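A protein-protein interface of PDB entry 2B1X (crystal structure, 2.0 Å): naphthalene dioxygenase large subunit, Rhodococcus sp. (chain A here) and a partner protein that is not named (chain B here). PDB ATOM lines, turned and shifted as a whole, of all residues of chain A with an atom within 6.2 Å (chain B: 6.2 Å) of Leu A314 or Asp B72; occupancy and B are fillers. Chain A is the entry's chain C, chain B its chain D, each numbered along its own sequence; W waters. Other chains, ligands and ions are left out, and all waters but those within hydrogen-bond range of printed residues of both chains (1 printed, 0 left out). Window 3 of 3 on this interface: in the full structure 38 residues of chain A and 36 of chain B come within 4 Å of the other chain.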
ATOM      1  N   LEU A 227     -17.451 -25.263 -18.171  1.00  0.00           N
ATOM      2  CA  LEU A 227     -16.143 -24.926 -18.708  1.00  0.00           C
ATOM      3  C   LEU A 227     -16.058 -23.463 -19.116  1.00  0.00           C
ATOM      4  O   LEU A 227     -14.987 -23.003 -19.468  1.00  0.00           O
ATOM      5  CB  LEU A 227     -15.755 -25.841 -19.903  1.00  0.00           C
ATOM      6  CG  LEU A 227     -15.585 -27.353 -19.654  1.00  0.00           C
ATOM      7  CD1 LEU A 227     -14.984 -28.070 -20.881  1.00  0.00           C
ATOM      8  CD2 LEU A 227     -14.761 -27.613 -18.440  1.00  0.00           C
ATOM      9  N   LEU A 229     -17.868 -22.146 -21.714  1.00  0.00           N
ATOM     10  CA  LEU A 229     -18.083 -22.012 -23.158  1.00  0.00           C
ATOM     11  C   LEU A 229     -19.525 -21.760 -23.562  1.00  0.00           C
ATOM     12  O   LEU A 229     -19.782 -21.149 -24.591  1.00  0.00           O
ATOM     13  CB  LEU A 229     -17.561 -23.221 -23.921  1.00  0.00           C
ATOM     14  CG  LEU A 229     -16.056 -23.255 -24.193  1.00  0.00           C
ATOM     15  CD1 LEU A 229     -15.460 -24.371 -23.380  1.00  0.00           C
ATOM     16  CD2 LEU A 229     -15.805 -23.478 -25.659  1.00  0.00           C
ATOM     17  N   ASP A 312     -11.820 -22.939 -27.110  1.00  0.00           N
ATOM     18  CA  ASP A 312     -11.446 -23.785 -25.989  1.00  0.00           C
ATOM     19  C   ASP A 312     -11.862 -23.052 -24.731  1.00  0.00           C
ATOM     20  O   ASP A 312     -12.416 -21.955 -24.815  1.00  0.00           O
ATOM     21  CB  ASP A 312      -9.946 -24.133 -26.007  1.00  0.00           C
ATOM     22  CG  ASP A 312      -9.049 -22.903 -25.890  1.00  0.00           C
ATOM     23  OD1 ASP A 312      -8.034 -22.844 -26.600  1.00  0.00           O
ATOM     24  OD2 ASP A 312      -9.276 -21.963 -25.113  1.00  0.00           O
ATOM     25  N   HIS A 313     -11.577 -23.634 -23.578  1.00  0.00           N
ATOM     26  CA  HIS A 313     -11.996 -23.073 -22.298  1.00  0.00           C
ATOM     27  C   HIS A 313     -11.216 -21.838 -21.826  1.00  0.00           C
ATOM     28  O   HIS A 313     -11.597 -21.231 -20.831  1.00  0.00           O
ATOM     29  CB  HIS A 313     -11.955 -24.156 -21.225  1.00  0.00           C
ATOM     30  CG  HIS A 313     -10.577 -24.681 -20.968  1.00  0.00           C
ATOM     31  ND1 HIS A 313      -9.839 -25.313 -21.939  1.00  0.00           N
ATOM     32  CD2 HIS A 313      -9.801 -24.660 -19.853  1.00  0.00           C
ATOM     33  CE1 HIS A 313      -8.668 -25.669 -21.439  1.00  0.00           C
ATOM     34  NE2 HIS A 313      -8.623 -25.286 -20.171  1.00  0.00           N
ATOM     35  N   LEU A 314     -10.154 -21.455 -22.538  1.00  0.00           N
ATOM     36  CA  LEU A 314      -9.316 -20.313 -22.111  1.00  0.00           C
ATOM     37  C   LEU A 314      -9.416 -19.088 -23.019  1.00  0.00           C
ATOM     38  O   LEU A 314      -8.822 -18.049 -22.717  1.00  0.00           O
ATOM     39  CB  LEU A 314      -7.848 -20.746 -21.998  1.00  0.00           C
ATOM     40  CG  LEU A 314      -7.514 -21.974 -21.147  1.00  0.00           C
ATOM     41  CD1 LEU A 314      -6.062 -22.423 -21.358  1.00  0.00           C
ATOM     42  CD2 LEU A 314      -7.748 -21.660 -19.736  1.00  0.00           C
ATOM     43  N   SER A 315     -10.180 -19.210 -24.106  1.00  0.00           N
ATOM     44  CA  SER A 315     -10.190 -18.214 -25.175  1.00  0.00           C
ATOM     45  C   SER A 315     -11.408 -17.302 -25.192  1.00  0.00           C
ATOM     46  O   SER A 315     -12.490 -17.712 -24.811  1.00  0.00           O
ATOM     47  CB  SER A 315     -10.040 -18.912 -26.518  1.00  0.00           C
ATOM     48  OG  SER A 315      -8.904 -19.756 -26.493  1.00  0.00           O
ATOM     49  N   ALA A 316     -11.206 -16.050 -25.621  1.00  0.00           N
ATOM     50  CA  ALA A 316     -12.304 -15.159 -25.978  1.00  0.00           C
ATOM     51  C   ALA A 316     -13.070 -15.752 -27.183  1.00  0.00           C
ATOM     52  O   ALA A 316     -12.481 -16.405 -28.053  1.00  0.00           O
ATOM     53  CB  ALA A 316     -11.773 -13.731 -26.312  1.00  0.00           C
ATOM     54  N   GLU B  40       3.461 -29.764 -25.238  1.00  0.00           N
ATOM     55  CA  GLU B  40       2.943 -28.426 -25.127  1.00  0.00           C
ATOM     56  C   GLU B  40       2.576 -27.858 -26.521  1.00  0.00           C
ATOM     57  O   GLU B  40       1.622 -27.076 -26.657  1.00  0.00           O
ATOM     58  CB  GLU B  40       4.002 -27.578 -24.413  1.00  0.00           C
ATOM     59  CG  GLU B  40       4.695 -28.288 -23.211  1.00  0.00           C
ATOM     60  CD  GLU B  40       5.705 -29.442 -23.537  1.00  0.00           C
ATOM     61  OE1 GLU B  40       6.287 -29.496 -24.650  1.00  0.00           O
ATOM     62  OE2 GLU B  40       5.941 -30.310 -22.632  1.00  0.00           O
ATOM     63  N   ASP B  70      -5.152 -28.556 -30.352  1.00  0.00           N
ATOM     64  CA  ASP B  70      -3.834 -28.254 -29.816  1.00  0.00           C
ATOM     65  C   ASP B  70      -3.870 -28.655 -28.342  1.00  0.00           C
ATOM     66  O   ASP B  70      -4.843 -29.292 -27.907  1.00  0.00           O
ATOM     67  CB  ASP B  70      -3.475 -26.781 -30.037  1.00  0.00           C
ATOM     68  CG  ASP B  70      -4.562 -25.818 -29.560  1.00  0.00           C
ATOM     69  OD1 ASP B  70      -5.328 -26.139 -28.614  1.00  0.00           O
ATOM     70  OD2 ASP B  70      -4.710 -24.687 -30.075  1.00  0.00           O
ATOM     71  N   ALA B  71      -2.840 -28.308 -27.564  1.00  0.00           N
ATOM     72  CA  ALA B  71      -2.802 -28.721 -26.157  1.00  0.00           C
ATOM     73  C   ALA B  71      -3.953 -28.126 -25.334  1.00  0.00           C
ATOM     74  O   ALA B  71      -4.508 -28.799 -24.481  1.00  0.00           O
ATOM     75  CB  ALA B  71      -1.458 -28.383 -25.522  1.00  0.00           C
ATOM     76  N   ASP B  72      -4.307 -26.874 -25.607  1.00  0.00           N
ATOM     77  CA  ASP B  72      -5.375 -26.200 -24.921  1.00  0.00           C
ATOM     78  C   ASP B  72      -6.759 -26.838 -25.230  1.00  0.00           C
ATOM     79  O   ASP B  72      -7.533 -27.047 -24.320  1.00  0.00           O
ATOM     80  CB  ASP B  72      -5.381 -24.721 -25.294  1.00  0.00           C
ATOM     81  CG  ASP B  72      -4.235 -23.917 -24.633  1.00  0.00           C
ATOM     82  OD1 ASP B  72      -3.563 -24.411 -23.691  1.00  0.00           O
ATOM     83  OD2 ASP B  72      -3.975 -22.752 -24.986  1.00  0.00           O
ATOM     84  N   SER B  73      -7.051 -27.158 -26.495  1.00  0.00           N
ATOM     85  CA  SER B  73      -8.358 -27.719 -26.842  1.00  0.00           C
ATOM     86  C   SER B  73      -8.465 -29.181 -26.412  1.00  0.00           C
ATOM     87  O   SER B  73      -9.541 -29.663 -26.019  1.00  0.00           O
ATOM     88  CB  SER B  73      -8.676 -27.543 -28.328  1.00  0.00           C
ATOM     89  OG  SER B  73      -7.748 -28.267 -29.105  1.00  0.00           O
ATOM     90  N   MET B  74      -7.343 -29.880 -26.436  1.00  0.00           N
ATOM     91  CA  MET B  74      -7.309 -31.257 -25.959  1.00  0.00           C
ATOM     92  C   MET B  74      -7.538 -31.294 -24.435  1.00  0.00           C
ATOM     93  O   MET B  74      -8.162 -32.226 -23.916  1.00  0.00           O
ATOM     94  CB  MET B  74      -5.975 -31.891 -26.345  1.00  0.00           C
ATOM     95  CG  MET B  74      -5.924 -33.391 -26.370  1.00  0.00           C
ATOM     96  SD  MET B  74      -7.343 -34.278 -27.178  1.00  0.00           S
ATOM     97  CE  MET B  74      -6.821 -34.414 -28.756  1.00  0.00           C
ATOM     98  N   GLU B  75      -7.024 -30.284 -23.714  1.00  0.00           N
ATOM     99  CA  GLU B  75      -7.314 -30.138 -22.281  1.00  0.00           C
ATOM    100  C   GLU B  75      -8.813 -29.900 -22.037  1.00  0.00           C
ATOM    101  O   GLU B  75      -9.408 -30.510 -21.148  1.00  0.00           O
ATOM    102  CB  GLU B  75      -6.521 -28.972 -21.680  1.00  0.00           C
ATOM    103  CG  GLU B  75      -6.655 -28.855 -20.173  1.00  0.00           C
ATOM    104  CD  GLU B  75      -5.801 -27.728 -19.584  1.00  0.00           C
ATOM    105  OE1 GLU B  75      -5.585 -26.691 -20.257  1.00  0.00           O
ATOM    106  OE2 GLU B  75      -5.332 -27.880 -18.444  1.00  0.00           O
ATOM    107  N   MET B  76      -9.409 -29.003 -22.836  1.00  0.00           N
ATOM    108  CA  MET B  76     -10.836 -28.743 -22.761  1.00  0.00           C
ATOM    109  C   MET B  76     -11.635 -30.049 -22.929  1.00  0.00           C
ATOM    110  O   MET B  76     -12.572 -30.317 -22.162  1.00  0.00           O
ATOM    111  CB  MET B  76     -11.238 -27.732 -23.834  1.00  0.00           C
ATOM    112  CG  MET B  76     -12.655 -27.239 -23.694  1.00  0.00           C
ATOM    113  SD  MET B  76     -13.566 -27.439 -25.246  1.00  0.00           S
ATOM    114  CE  MET B  76     -13.980 -28.968 -25.136  1.00  0.00           C
ATOM    115  N   ARG B  77     -11.249 -30.842 -23.937  1.00  0.00           N
ATOM    116  CA  ARG B  77     -11.862 -32.141 -24.261  1.00  0.00           C
ATOM    117  C   ARG B  77     -11.865 -33.081 -23.043  1.00  0.00           C
ATOM    118  O   ARG B  77     -12.905 -33.681 -22.672  1.00  0.00           O
ATOM    119  CB  ARG B  77     -11.136 -32.756 -25.492  1.00  0.00           C
ATOM    120  CG  ARG B  77     -11.902 -33.836 -26.256  1.00  0.00           C
ATOM    121  CD  ARG B  77     -11.274 -34.268 -27.602  1.00  0.00           C
ATOM    122  NE  ARG B  77     -11.129 -33.136 -28.549  1.00  0.00           N
ATOM    123  CZ  ARG B  77     -12.121 -32.638 -29.305  1.00  0.00           C
ATOM    124  NH1 ARG B  77     -13.358 -33.147 -29.244  1.00  0.00           N
ATOM    125  NH2 ARG B  77     -11.877 -31.630 -30.140  1.00  0.00           N
HETATM  126  O   HOH W   1      -7.046 -24.128 -28.731  1.00  0.00           O
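Asp B72 touches just these residues of chain A: Asp A312 (3.5 Å), His A313 (3.4 Å) and Leu A314 (3.95 Å). Of the printed residues of chain A, Glu B75 touches His A313. Of the printed residues of chain A, Met B76 touches Leu A227 (3.5 Å) and His A313 (3.4 Å). The nearest residue of chain B that does not touch Leu A314 is Glu B75 (4.4 Å). The nearest residue of chain A that does not touch Asp B72 is Ser A315 (6.0 Å). The nearest printed residue of chain A that does not touch Met B76 is Leu A229 (4.02 Å).
Among the printed residues, merely in contact across the chains: His A313 with Met B76 (3.4 Å), His A313 with Asp B72 (3.4 Å), Asp A312 with Asp B72 (3.5 Å), Leu A227 with Met B76 (3.5 Å) and Leu A314 with Asp B72 (3.95 Å).
NE2 of His A313 is in hydrogen-bond range of OE1 of Glu B75 (3.3 Å).
OD1 of Asp B70 lies within hydrogen-bond range of N of Asp B72 (3.3 Å). OD2 of Asp A312 sits at hydrogen-bond distance from N of Leu A314, 2.8 Å away. The side-chain hydroxyl of Ser A315 is in hydrogen-bond range of the side-chain carboxylate of Asp A312, 2.6 Å away.
Of the 7 printed residues of chain A, 4 touch a printed residue of chain B. Printed residues of chain A that touch a printed residue of chain B: Leu A227, Asp A312, His A313 and Leu A314. Hydrophobic or aromatic side chains of chain A that line the printed part of chain B: Leu A227, His A313 and Leu A314. Printed residues of chain B that touch a printed residue of chain A: Asp B72, Glu B75 and Met B76. Among the printed residues, 6 pairs touch across the chains.
Water W1 bridges the side-chain carboxylate (OD1) of Asp B70 and the side-chain carboxylate (OD1) of Asp A312.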
